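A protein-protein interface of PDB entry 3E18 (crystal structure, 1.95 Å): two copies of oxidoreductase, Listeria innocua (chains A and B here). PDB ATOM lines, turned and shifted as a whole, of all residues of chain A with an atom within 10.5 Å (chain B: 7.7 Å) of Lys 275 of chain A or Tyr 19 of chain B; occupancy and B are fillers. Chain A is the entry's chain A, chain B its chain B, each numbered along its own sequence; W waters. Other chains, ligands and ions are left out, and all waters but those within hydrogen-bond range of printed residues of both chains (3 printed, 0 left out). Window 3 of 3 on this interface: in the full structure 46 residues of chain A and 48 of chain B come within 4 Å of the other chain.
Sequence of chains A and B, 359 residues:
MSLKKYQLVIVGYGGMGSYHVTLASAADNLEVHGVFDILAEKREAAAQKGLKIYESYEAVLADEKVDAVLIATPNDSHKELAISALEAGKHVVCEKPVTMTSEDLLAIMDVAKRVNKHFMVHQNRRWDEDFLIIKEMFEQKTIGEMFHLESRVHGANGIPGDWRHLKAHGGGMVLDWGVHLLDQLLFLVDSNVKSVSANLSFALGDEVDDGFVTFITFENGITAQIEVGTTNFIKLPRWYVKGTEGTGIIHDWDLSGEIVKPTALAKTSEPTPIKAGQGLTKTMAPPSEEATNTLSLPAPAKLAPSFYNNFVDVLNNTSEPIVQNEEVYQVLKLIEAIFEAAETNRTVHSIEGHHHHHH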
ATOM      1  N   THR A 272      -7.518  42.814  -5.131  1.00  0.00           N
ATOM      2  CA  THR A 272      -6.910  41.681  -4.441  1.00  0.00           C
ATOM      3  C   THR A 272      -7.953  40.563  -4.327  1.00  0.00           C
ATOM      4  O   THR A 272      -9.063  40.800  -3.837  1.00  0.00           O
ATOM      5  CB  THR A 272      -6.329  42.064  -3.048  1.00  0.00           C
ATOM      6  OG1 THR A 272      -7.337  42.702  -2.255  1.00  0.00           O
ATOM      7  CG2 THR A 272      -5.137  43.006  -3.198  1.00  0.00           C
ATOM      8  N   PRO A 273      -7.607  39.352  -4.816  1.00  0.00           N
ATOM      9  CA  PRO A 273      -8.532  38.215  -4.862  1.00  0.00           C
ATOM     10  C   PRO A 273      -9.104  37.762  -3.517  1.00  0.00           C
ATOM     11  O   PRO A 273      -8.487  37.980  -2.467  1.00  0.00           O
ATOM     12  CB  PRO A 273      -7.690  37.094  -5.493  1.00  0.00           C
ATOM     13  CG  PRO A 273      -6.279  37.519  -5.335  1.00  0.00           C
ATOM     14  CD  PRO A 273      -6.297  39.008  -5.399  1.00  0.00           C
ATOM     15  N   ILE A 274     -10.300  37.172  -3.563  1.00  0.00           N
ATOM     16  CA  ILE A 274     -10.874  36.485  -2.407  1.00  0.00           C
ATOM     17  C   ILE A 274     -11.160  35.025  -2.740  1.00  0.00           C
ATOM     18  O   ILE A 274     -11.112  34.608  -3.906  1.00  0.00           O
ATOM     19  CB  ILE A 274     -12.229  37.083  -1.913  1.00  0.00           C
ATOM     20  CG1 ILE A 274     -12.760  38.179  -2.840  1.00  0.00           C
ATOM     21  CG2 ILE A 274     -12.138  37.470  -0.425  1.00  0.00           C
ATOM     22  CD1 ILE A 274     -14.265  38.128  -3.015  1.00  0.00           C
ATOM     23  N   LYS A 275     -11.452  34.265  -1.688  1.00  0.00           N
ATOM     24  CA  LYS A 275     -12.051  32.949  -1.799  1.00  0.00           C
ATOM     25  C   LYS A 275     -13.543  33.161  -2.082  1.00  0.00           C
ATOM     26  O   LYS A 275     -14.287  33.659  -1.227  1.00  0.00           O
ATOM     27  CB  LYS A 275     -11.846  32.175  -0.486  1.00  0.00           C
ATOM     28  CG  LYS A 275     -12.549  30.808  -0.389  1.00  0.00           C
ATOM     29  CD  LYS A 275     -11.582  29.625  -0.535  1.00  0.00           C
ATOM     30  CE  LYS A 275     -11.338  29.244  -1.993  1.00  0.00           C
ATOM     31  NZ  LYS A 275     -10.462  28.049  -2.103  1.00  0.00           N
ATOM     32  N   ALA A 276     -13.966  32.809  -3.293  1.00  0.00           N
ATOM     33  CA  ALA A 276     -15.382  32.808  -3.640  1.00  0.00           C
ATOM     34  C   ALA A 276     -15.803  31.369  -3.909  1.00  0.00           C
ATOM     35  O   ALA A 276     -15.507  30.829  -4.969  1.00  0.00           O
ATOM     36  CB  ALA A 276     -15.625  33.665  -4.861  1.00  0.00           C
ATOM     37  N   GLY A 277     -16.480  30.752  -2.944  1.00  0.00           N
ATOM     38  CA  GLY A 277     -16.826  29.333  -3.037  1.00  0.00           C
ATOM     39  C   GLY A 277     -15.573  28.476  -3.150  1.00  0.00           C
ATOM     40  O   GLY A 277     -14.667  28.588  -2.322  1.00  0.00           O
ATOM     41  N   GLN A 278     -15.503  27.662  -4.204  1.00  0.00           N
ATOM     42  CA  GLN A 278     -14.387  26.723  -4.398  1.00  0.00           C
ATOM     43  C   GLN A 278     -13.196  27.288  -5.162  1.00  0.00           C
ATOM     44  O   GLN A 278     -12.220  26.572  -5.402  1.00  0.00           O
ATOM     45  CB  GLN A 278     -14.863  25.439  -5.092  1.00  0.00           C
ATOM     46  CG  GLN A 278     -15.837  24.619  -4.285  1.00  0.00           C
ATOM     47  CD  GLN A 278     -15.216  24.007  -3.037  1.00  0.00           C
ATOM     48  OE1 GLN A 278     -14.592  22.954  -3.096  1.00  0.00           O
ATOM     49  NE2 GLN A 278     -15.398  24.665  -1.903  1.00  0.00           N
ATOM     50  N   GLY A 279     -13.268  28.561  -5.532  1.00  0.00           N
ATOM     51  CA  GLY A 279     -12.234  29.161  -6.366  1.00  0.00           C
ATOM     52  C   GLY A 279     -11.798  30.548  -5.945  1.00  0.00           C
ATOM     53  O   GLY A 279     -12.511  31.254  -5.229  1.00  0.00           O
ATOM     54  N   LEU A 280     -10.608  30.926  -6.392  1.00  0.00           N
ATOM     55  CA  LEU A 280     -10.103  32.271  -6.192  1.00  0.00           C
ATOM     56  C   LEU A 280     -10.574  33.147  -7.343  1.00  0.00           C
ATOM     57  O   LEU A 280     -10.506  32.741  -8.508  1.00  0.00           O
ATOM     58  CB  LEU A 280      -8.573  32.269  -6.106  1.00  0.00           C
ATOM     59  CG  LEU A 280      -7.967  31.677  -4.829  1.00  0.00           C
ATOM     60  CD1 LEU A 280      -6.522  31.258  -5.061  1.00  0.00           C
ATOM     61  CD2 LEU A 280      -8.078  32.647  -3.654  1.00  0.00           C
ATOM     62  N   THR A 281     -11.065  34.339  -7.012  1.00  0.00           N
ATOM     63  CA  THR A 281     -11.530  35.281  -8.034  1.00  0.00           C
ATOM     64  C   THR A 281     -10.942  36.684  -7.885  1.00  0.00           C
ATOM     65  O   THR A 281     -10.879  37.235  -6.785  1.00  0.00           O
ATOM     66  CB  THR A 281     -13.087  35.360  -8.115  1.00  0.00           C
ATOM     67  OG1 THR A 281     -13.468  36.168  -9.239  1.00  0.00           O
ATOM     68  CG2 THR A 281     -13.702  35.940  -6.824  1.00  0.00           C
ATOM     69  N   LYS A 282     -10.524  37.245  -9.015  1.00  0.00           N
ATOM     70  CA  LYS A 282     -10.071  38.626  -9.085  1.00  0.00           C
ATOM     71  C   LYS A 282     -11.202  39.501  -9.656  1.00  0.00           C
ATOM     72  O   LYS A 282     -11.519  40.549  -9.102  1.00  0.00           O
ATOM     73  CB  LYS A 282      -8.807  38.706  -9.949  1.00  0.00           C
ATOM     74  CG  LYS A 282      -7.811  39.791  -9.554  1.00  0.00           C
ATOM     75  CD  LYS A 282      -6.511  39.640 -10.349  1.00  0.00           C
ATOM     76  CE  LYS A 282      -5.759  40.963 -10.497  1.00  0.00           C
ATOM     77  NZ  LYS A 282      -5.037  41.366  -9.258  1.00  0.00           N
ATOM     78  N   THR A 283     -11.819  39.039 -10.747  1.00  0.00           N
ATOM     79  CA  THR A 283     -12.883  39.775 -11.453  1.00  0.00           C
ATOM     80  C   THR A 283     -14.172  39.987 -10.639  1.00  0.00           C
ATOM     81  O   THR A 283     -14.871  40.972 -10.840  1.00  0.00           O
ATOM     82  CB  THR A 283     -13.218  39.114 -12.811  1.00  0.00           C
ATOM     83  OG1 THR A 283     -14.457  39.629 -13.325  1.00  0.00           O
ATOM     84  CG2 THR A 283     -13.343  37.628 -12.649  1.00  0.00           C
ATOM     85  N   MET A 284     -14.474  39.069  -9.725  1.00  0.00           N
ATOM     86  CA  MET A 284     -15.661  39.191  -8.878  1.00  0.00           C
ATOM     87  C   MET A 284     -15.310  39.603  -7.443  1.00  0.00           C
ATOM     88  O   MET A 284     -16.163  39.583  -6.548  1.00  0.00           O
ATOM     89  CB  MET A 284     -16.493  37.895  -8.920  1.00  0.00           C
ATOM     90  CG  MET A 284     -16.954  37.520 -10.335  1.00  0.00           C
ATOM     91  SD  MET A 284     -18.009  38.764 -11.135  1.00  0.00           S
ATOM     92  CE  MET A 284     -18.443  37.858 -12.630  1.00  0.00           C
ATOM     93  N   ALA A 285     -14.048  39.982  -7.240  1.00  0.00           N
ATOM     94  CA  ALA A 285     -13.577  40.533  -5.964  1.00  0.00           C
ATOM     95  C   ALA A 285     -13.922  42.022  -5.892  1.00  0.00           C
ATOM     96  O   ALA A 285     -14.020  42.674  -6.940  1.00  0.00           O
ATOM     97  CB  ALA A 285     -12.072  40.335  -5.841  1.00  0.00           C
ATOM     98  N   PRO A 286     -14.112  42.574  -4.666  1.00  0.00           N
ATOM     99  CA  PRO A 286     -14.307  44.025  -4.579  1.00  0.00           C
ATOM    100  C   PRO A 286     -13.167  44.779  -5.270  1.00  0.00           C
ATOM    101  O   PRO A 286     -12.014  44.338  -5.201  1.00  0.00           O
ATOM    102  CB  PRO A 286     -14.277  44.295  -3.071  1.00  0.00           C
ATOM    103  CG  PRO A 286     -14.715  43.020  -2.452  1.00  0.00           C
ATOM    104  CD  PRO A 286     -14.171  41.937  -3.336  1.00  0.00           C
ATOM    105  N   ILE B  10      -0.614  18.804 -16.471  1.00  0.00           N
ATOM    106  CA  ILE B  10      -1.369  20.043 -16.674  1.00  0.00           C
ATOM    107  C   ILE B  10      -1.036  20.617 -18.042  1.00  0.00           C
ATOM    108  O   ILE B  10       0.125  20.862 -18.352  1.00  0.00           O
ATOM    109  CB  ILE B  10      -1.046  21.106 -15.603  1.00  0.00           C
ATOM    110  CG1 ILE B  10      -1.206  20.557 -14.174  1.00  0.00           C
ATOM    111  CG2 ILE B  10      -1.891  22.385 -15.800  1.00  0.00           C
ATOM    112  CD1 ILE B  10      -2.573  20.081 -13.833  1.00  0.00           C
ATOM    113  N   GLY B  12      -1.650  23.818 -20.007  1.00  0.00           N
ATOM    114  CA  GLY B  12      -2.090  25.202 -19.849  1.00  0.00           C
ATOM    115  C   GLY B  12      -1.812  25.602 -18.424  1.00  0.00           C
ATOM    116  O   GLY B  12      -2.599  25.305 -17.523  1.00  0.00           O
ATOM    117  N   TYR B  13      -0.670  26.245 -18.211  1.00  0.00           N
ATOM    118  CA  TYR B  13      -0.226  26.592 -16.867  1.00  0.00           C
ATOM    119  C   TYR B  13      -0.474  28.075 -16.600  1.00  0.00           C
ATOM    120  O   TYR B  13       0.418  28.817 -16.201  1.00  0.00           O
ATOM    121  CB  TYR B  13       1.251  26.220 -16.670  1.00  0.00           C
ATOM    122  CG  TYR B  13       1.693  26.209 -15.217  1.00  0.00           C
ATOM    123  CD1 TYR B  13       1.386  25.137 -14.379  1.00  0.00           C
ATOM    124  CD2 TYR B  13       2.437  27.267 -14.690  1.00  0.00           C
ATOM    125  CE1 TYR B  13       1.799  25.132 -13.043  1.00  0.00           C
ATOM    126  CE2 TYR B  13       2.837  27.278 -13.362  1.00  0.00           C
ATOM    127  CZ  TYR B  13       2.523  26.211 -12.550  1.00  0.00           C
ATOM    128  OH  TYR B  13       2.937  26.242 -11.240  1.00  0.00           O
ATOM    129  N   GLY B  14      -1.700  28.513 -16.839  1.00  0.00           N
ATOM    130  CA  GLY B  14      -2.064  29.896 -16.589  1.00  0.00           C
ATOM    131  C   GLY B  14      -2.633  29.996 -15.192  1.00  0.00           C
ATOM    132  O   GLY B  14      -2.212  29.255 -14.297  1.00  0.00           O
ATOM    133  N   GLY B  15      -3.601  30.898 -15.019  1.00  0.00           N
ATOM    134  CA  GLY B  15      -4.244  31.137 -13.730  1.00  0.00           C
ATOM    135  C   GLY B  15      -4.912  29.930 -13.098  1.00  0.00           C
ATOM    136  O   GLY B  15      -4.645  29.613 -11.939  1.00  0.00           O
ATOM    137  N   MET B  16      -5.781  29.253 -13.849  1.00  0.00           N
ATOM    138  CA  MET B  16      -6.458  28.059 -13.328  1.00  0.00           C
ATOM    139  C   MET B  16      -5.575  26.813 -13.381  1.00  0.00           C
ATOM    140  O   MET B  16      -5.556  26.036 -12.441  1.00  0.00           O
ATOM    141  CB  MET B  16      -7.789  27.803 -14.040  1.00  0.00           C
ATOM    142  CG  MET B  16      -8.697  26.836 -13.305  1.00  0.00           C
ATOM    143  SD  MET B  16      -9.057  27.382 -11.618  1.00  0.00           S
ATOM    144  CE  MET B  16      -9.855  25.922 -10.973  1.00  0.00           C
ATOM    145  N   GLY B  17      -4.844  26.628 -14.482  1.00  0.00           N
ATOM    146  CA  GLY B  17      -3.893  25.513 -14.599  1.00  0.00           C
ATOM    147  C   GLY B  17      -2.896  25.395 -13.449  1.00  0.00           C
ATOM    148  O   GLY B  17      -2.669  24.294 -12.950  1.00  0.00           O
ATOM    149  N   SER B  18      -2.316  26.514 -13.013  1.00  0.00           N
ATOM    150  CA  SER B  18      -1.378  26.479 -11.881  1.00  0.00           C
ATOM    151  C   SER B  18      -2.059  26.163 -10.548  1.00  0.00           C
ATOM    152  O   SER B  18      -1.437  25.586  -9.646  1.00  0.00           O
ATOM    153  CB  SER B  18      -0.585  27.777 -11.769  1.00  0.00           C
ATOM    154  OG  SER B  18      -1.433  28.904 -11.765  1.00  0.00           O
ATOM    155  N   TYR B  19      -3.329  26.549 -10.428  1.00  0.00           N
ATOM    156  CA  TYR B  19      -4.125  26.249  -9.224  1.00  0.00           C
ATOM    157  C   TYR B  19      -4.536  24.771  -9.143  1.00  0.00           C
ATOM    158  O   TYR B  19      -4.776  24.235  -8.050  1.00  0.00           O
ATOM    159  CB  TYR B  19      -5.357  27.164  -9.141  1.00  0.00           C
ATOM    160  CG  TYR B  19      -6.206  26.956  -7.900  1.00  0.00           C
ATOM    161  CD1 TYR B  19      -5.671  27.145  -6.626  1.00  0.00           C
ATOM    162  CD2 TYR B  19      -7.541  26.568  -8.003  1.00  0.00           C
ATOM    163  CE1 TYR B  19      -6.444  26.948  -5.481  1.00  0.00           C
ATOM    164  CE2 TYR B  19      -8.327  26.376  -6.871  1.00  0.00           C
ATOM    165  CZ  TYR B  19      -7.771  26.567  -5.612  1.00  0.00           C
ATOM    166  OH  TYR B  19      -8.532  26.380  -4.481  1.00  0.00           O
ATOM    167  N   HIS B  20      -4.613  24.115 -10.297  1.00  0.00           N
ATOM    168  CA  HIS B  20      -4.918  22.682 -10.360  1.00  0.00           C
ATOM    169  C   HIS B  20      -3.804  21.810  -9.812  1.00  0.00           C
ATOM    170  O   HIS B  20      -4.060  20.669  -9.451  1.00  0.00           O
ATOM    171  CB  HIS B  20      -5.208  22.253 -11.797  1.00  0.00           C
ATOM    172  CG  HIS B  20      -6.658  22.308 -12.155  1.00  0.00           C
ATOM    173  ND1 HIS B  20      -7.518  21.258 -11.924  1.00  0.00           N
ATOM    174  CD2 HIS B  20      -7.402  23.291 -12.714  1.00  0.00           C
ATOM    175  CE1 HIS B  20      -8.728  21.585 -12.340  1.00  0.00           C
ATOM    176  NE2 HIS B  20      -8.687  22.817 -12.814  1.00  0.00           N
ATOM    177  N   VAL B  21      -2.577  22.336  -9.744  1.00  0.00           N
ATOM    178  CA  VAL B  21      -1.479  21.607  -9.084  1.00  0.00           C
ATOM    179  C   VAL B  21      -1.865  21.390  -7.614  1.00  0.00           C
ATOM    180  O   VAL B  21      -1.788  20.271  -7.107  1.00  0.00           O
ATOM    181  CB  VAL B  21      -0.087  22.307  -9.225  1.00  0.00           C
ATOM    182  CG1 VAL B  21       1.017  21.441  -8.609  1.00  0.00           C
ATOM    183  CG2 VAL B  21       0.257  22.590 -10.688  1.00  0.00           C
ATOM    184  N   THR B  22      -2.343  22.448  -6.964  1.00  0.00           N
ATOM    185  CA  THR B  22      -2.854  22.377  -5.590  1.00  0.00           C
ATOM    186  C   THR B  22      -4.043  21.417  -5.448  1.00  0.00           C
ATOM    187  O   THR B  22      -3.999  20.508  -4.623  1.00  0.00           O
ATOM    188  CB  THR B  22      -3.229  23.785  -5.052  1.00  0.00           C
ATOM    189  OG1 THR B  22      -2.077  24.637  -5.098  1.00  0.00           O
ATOM    190  CG2 THR B  22      -3.763  23.713  -3.598  1.00  0.00           C
ATOM    191  N   LEU B  23      -5.082  21.622  -6.267  1.00  0.00           N
ATOM    192  CA  LEU B  23      -6.301  20.793  -6.285  1.00  0.00           C
ATOM    193  C   LEU B  23      -6.058  19.295  -6.515  1.00  0.00           C
ATOM    194  O   LEU B  23      -6.545  18.451  -5.744  1.00  0.00           O
ATOM    195  CB  LEU B  23      -7.281  21.316  -7.352  1.00  0.00           C
ATOM    196  CG  LEU B  23      -8.035  22.629  -7.091  1.00  0.00           C
ATOM    197  CD1 LEU B  23      -8.962  22.965  -8.259  1.00  0.00           C
ATOM    198  CD2 LEU B  23      -8.849  22.575  -5.786  1.00  0.00           C
ATOM    199  N   ALA B  24      -5.309  18.974  -7.569  1.00  0.00           N
ATOM    200  CA  ALA B  24      -5.035  17.591  -7.935  1.00  0.00           C
ATOM    201  C   ALA B  24      -4.183  16.886  -6.885  1.00  0.00           C
ATOM    202  O   ALA B  24      -4.452  15.735  -6.554  1.00  0.00           O
ATOM    203  CB  ALA B  24      -4.370  17.515  -9.301  1.00  0.00           C
ATOM    204  N   SER B  25      -3.187  17.588  -6.341  1.00  0.00           N
ATOM    205  CA  SER B  25      -2.303  17.012  -5.323  1.00  0.00           C
ATOM    206  C   SER B  25      -3.028  16.742  -4.010  1.00  0.00           C
ATOM    207  O   SER B  25      -2.564  15.934  -3.206  1.00  0.00           O
ATOM    208  CB  SER B  25      -1.100  17.917  -5.053  1.00  0.00           C
ATOM    209  OG  SER B  25      -0.392  18.195  -6.246  1.00  0.00           O
ATOM    210  N   LEU B  70      -4.967  17.324 -17.691  1.00  0.00           N
ATOM    211  CA  LEU B  70      -5.881  18.390 -17.326  1.00  0.00           C
ATOM    212  C   LEU B  70      -5.718  19.467 -18.388  1.00  0.00           C
ATOM    213  O   LEU B  70      -4.608  19.924 -18.625  1.00  0.00           O
ATOM    214  CB  LEU B  70      -5.545  18.923 -15.931  1.00  0.00           C
ATOM    215  CG  LEU B  70      -6.344  20.062 -15.262  1.00  0.00           C
ATOM    216  CD1 LEU B  70      -5.750  21.432 -15.552  1.00  0.00           C
ATOM    217  CD2 LEU B  70      -7.826  20.051 -15.610  1.00  0.00           C
ATOM    218  N   GLU B  95     -11.362  21.831 -18.254  1.00  0.00           N
ATOM    219  CA  GLU B  95     -11.947  23.022 -17.659  1.00  0.00           C
ATOM    220  C   GLU B  95     -13.225  23.460 -18.362  1.00  0.00           C
ATOM    221  O   GLU B  95     -13.404  23.218 -19.559  1.00  0.00           O
ATOM    222  CB  GLU B  95     -10.954  24.193 -17.597  1.00  0.00           C
ATOM    223  CG  GLU B  95     -10.208  24.332 -16.264  1.00  0.00           C
ATOM    224  CD  GLU B  95     -11.124  24.479 -15.047  1.00  0.00           C
ATOM    225  OE1 GLU B  95     -12.319  24.809 -15.184  1.00  0.00           O
ATOM    226  OE2 GLU B  95     -10.634  24.264 -13.931  1.00  0.00           O
ATOM    227  N   HIS B 122     -14.575  19.929 -15.441  1.00  0.00           N
ATOM    228  CA  HIS B 122     -14.276  20.470 -14.110  1.00  0.00           C
ATOM    229  C   HIS B 122     -15.364  21.430 -13.582  1.00  0.00           C
ATOM    230  O   HIS B 122     -15.165  22.647 -13.514  1.00  0.00           O
ATOM    231  CB  HIS B 122     -12.868  21.103 -14.041  1.00  0.00           C
ATOM    232  CG  HIS B 122     -12.420  21.439 -12.643  1.00  0.00           C
ATOM    233  ND1 HIS B 122     -11.844  22.645 -12.314  1.00  0.00           N
ATOM    234  CD2 HIS B 122     -12.480  20.726 -11.494  1.00  0.00           C
ATOM    235  CE1 HIS B 122     -11.560  22.657 -11.021  1.00  0.00           C
ATOM    236  NE2 HIS B 122     -11.939  21.505 -10.499  1.00  0.00           N
ATOM    237  N   ASN B 124     -16.354  22.478 -10.686  1.00  0.00           N
ATOM    238  CA  ASN B 124     -15.965  22.616  -9.278  1.00  0.00           C
ATOM    239  C   ASN B 124     -16.956  23.369  -8.433  1.00  0.00           C
ATOM    240  O   ASN B 124     -16.963  23.217  -7.208  1.00  0.00           O
ATOM    241  CB  ASN B 124     -14.578  23.289  -9.127  1.00  0.00           C
ATOM    242  CG  ASN B 124     -14.487  24.653  -9.826  1.00  0.00           C
ATOM    243  OD1 ASN B 124     -14.932  24.820 -10.964  1.00  0.00           O
ATOM    244  ND2 ASN B 124     -13.894  25.629  -9.147  1.00  0.00           N
ATOM    245  N   ARG B 125     -17.793  24.190  -9.073  1.00  0.00           N
ATOM    246  CA  ARG B 125     -18.708  25.031  -8.305  1.00  0.00           C
ATOM    247  C   ARG B 125     -19.981  24.345  -7.797  1.00  0.00           C
ATOM    248  O   ARG B 125     -20.748  24.953  -7.065  1.00  0.00           O
ATOM    249  CB  ARG B 125     -18.970  26.379  -8.993  1.00  0.00           C
ATOM    250  CG  ARG B 125     -17.699  27.242  -9.018  1.00  0.00           C
ATOM    251  CD  ARG B 125     -17.954  28.726  -9.251  1.00  0.00           C
ATOM    252  NE  ARG B 125     -16.721  29.513  -9.056  1.00  0.00           N
ATOM    253  CZ  ARG B 125     -16.332  30.029  -7.894  1.00  0.00           C
ATOM    254  NH1 ARG B 125     -17.062  29.848  -6.794  1.00  0.00           N
ATOM    255  NH2 ARG B 125     -15.210  30.736  -7.827  1.00  0.00           N
ATOM    256  N   TRP B 253     -20.525  35.787  -0.816  1.00  0.00           N
ATOM    257  CA  TRP B 253     -19.632  34.654  -0.637  1.00  0.00           C
ATOM    258  C   TRP B 253     -19.256  34.351   0.818  1.00  0.00           C
ATOM    259  O   TRP B 253     -18.789  33.253   1.122  1.00  0.00           O
ATOM    260  CB  TRP B 253     -18.362  34.894  -1.441  1.00  0.00           C
ATOM    261  CG  TRP B 253     -18.587  35.117  -2.914  1.00  0.00           C
ATOM    262  CD1 TRP B 253     -18.413  36.281  -3.602  1.00  0.00           C
ATOM    263  CD2 TRP B 253     -19.018  34.144  -3.871  1.00  0.00           C
ATOM    264  NE1 TRP B 253     -18.703  36.096  -4.936  1.00  0.00           N
ATOM    265  CE2 TRP B 253     -19.071  34.790  -5.130  1.00  0.00           C
ATOM    266  CE3 TRP B 253     -19.347  32.783  -3.795  1.00  0.00           C
ATOM    267  CZ2 TRP B 253     -19.454  34.123  -6.304  1.00  0.00           C
ATOM    268  CZ3 TRP B 253     -19.725  32.124  -4.957  1.00  0.00           C
ATOM    269  CH2 TRP B 253     -19.769  32.795  -6.198  1.00  0.00           C
ATOM    270  N   ASP B 254     -19.471  35.316   1.710  1.00  0.00           N
ATOM    271  CA  ASP B 254     -19.229  35.119   3.145  1.00  0.00           C
ATOM    272  C   ASP B 254     -20.340  34.313   3.821  1.00  0.00           C
ATOM    273  O   ASP B 254     -20.286  34.049   5.027  1.00  0.00           O
ATOM    274  CB  ASP B 254     -19.004  36.469   3.854  1.00  0.00           C
ATOM    275  CG  ASP B 254     -20.226  37.404   3.791  1.00  0.00           C
ATOM    276  OD1 ASP B 254     -21.197  37.129   3.040  1.00  0.00           O
ATOM    277  OD2 ASP B 254     -20.207  38.435   4.508  1.00  0.00           O
ATOM    278  N   TYR B 308     -11.716  15.709  -7.471  1.00  0.00           N
ATOM    279  CA  TYR B 308     -10.570  14.917  -7.888  1.00  0.00           C
ATOM    280  C   TYR B 308     -10.534  13.513  -7.289  1.00  0.00           C
ATOM    281  O   TYR B 308     -10.065  12.576  -7.940  1.00  0.00           O
ATOM    282  CB  TYR B 308      -9.278  15.676  -7.653  1.00  0.00           C
ATOM    283  CG  TYR B 308      -8.854  16.485  -8.858  1.00  0.00           C
ATOM    284  CD1 TYR B 308      -8.733  17.869  -8.787  1.00  0.00           C
ATOM    285  CD2 TYR B 308      -8.604  15.861 -10.071  1.00  0.00           C
ATOM    286  CE1 TYR B 308      -8.346  18.608  -9.894  1.00  0.00           C
ATOM    287  CE2 TYR B 308      -8.206  16.583 -11.192  1.00  0.00           C
ATOM    288  CZ  TYR B 308      -8.076  17.955 -11.094  1.00  0.00           C
ATOM    289  OH  TYR B 308      -7.685  18.662 -12.197  1.00  0.00           O
HETATM  290  O   HOH W   1     -17.304  31.392  -0.316  1.00  0.00           O
HETATM  291  O   HOH W   2     -18.814  38.809  -6.633  1.00  0.00           O
HETATM  292  O   HOH W   3     -14.860  21.765  -6.125  1.00  0.00           O
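Among the printed residues, merely in contact across the chains: Ala 276 of chain A with Trp 253 of chain B, Gly 277 of chain A with Arg 125 of chain B, Gly 277 of chain A with Trp 253 of chain B, Gln 278 of chain A with Tyr 19 of chain B, Gln 278 of chain A with Asn 124 of chain B, Gln 278 of chain A with Arg 125 of chain B and Gly 279 of chain A with Arg 125 of chain B.
Water W2 lies within hydrogen-bond range of O of Met 284 of chain A (2.8 Å) and NE1 of Trp 253 of chain B (3.2 Å).
Water W3 bridges O of Asn 124 of chain B and OE1 of Gln 278 of chain A.
Water W1 bridges the backbone carbonyl oxygen (O) of Trp 253 of chain B (2.8 Å) and the backbone NH (N) of Gly 277 of chain A (2.8 Å).
Thr 272 of chain A touches none of the printed residues of chain B.
Lys 275 of chain A touches just one residue of chain B: Tyr 19.
Of the printed residues of chain B, Gly 277 of chain A touches Arg 125 and Trp 253.
Of the printed residues of chain B, Gln 278 of chain A touches Tyr 19 (3.8 Å), Asn 124 (3.4 Å) and Arg 125 (3.7 Å).
Of the printed residues of chain B, Gly 279 of chain A touches Arg 125 (3.7 Å).
Gly 12 of chain B touches none of the printed residues of chain A.
Met 16 of chain B touches none of the printed residues of chain A.
No residue of chain A comes within 4 Å of Gly 17 of chain B.
No residue of chain A comes within 4 Å of His 20 of chain B.
No residue of chain A comes within 4 Å of Thr 22 of chain B.
Of the printed residues of chain A, Asn 124 of chain B touches Gln 278.
Printed residues of chain A within 4 Å of Arg 125 of chain B: Ala 276 (2.6 Å), Gly 277 (3.8 Å), Gln 278 (3.7 Å) and Gly 279 (3.7 Å).
The nearest printed residue of chain B that does not touch Gly 279 of chain A is Asn 124 of chain B (4.7 Å).
No position is printed for both chains.
The side-chain amino group (NZ) of Lys 275 of chain A sits at hydrogen-bond distance from the side-chain hydroxyl (OH) of Tyr 19 of chain B, 3.5 Å away.
NH1 of Arg 125 of chain B sits at hydrogen-bond distance from O of Ala 276 of chain A (2.6 Å).
The backbone carbonyl oxygen of His 122 of chain B lies close to the side-chain amide oxygen of Asn 124 of chain B (3.4 Å).
Of the 15 printed residues of chain A, 5 touch a printed residue of chain B.
Hydrophobic or aromatic side chains of chain A that line the printed part of chain B: Ala 276.
Hydrophobic or aromatic side chains of chain B that line the printed part of chain A: Tyr 19 and Trp 253.
Among the printed residues, no Asp or Glu carboxylate lies within 4 Å of a Lys or Arg side-chain nitrogen of the other chain.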
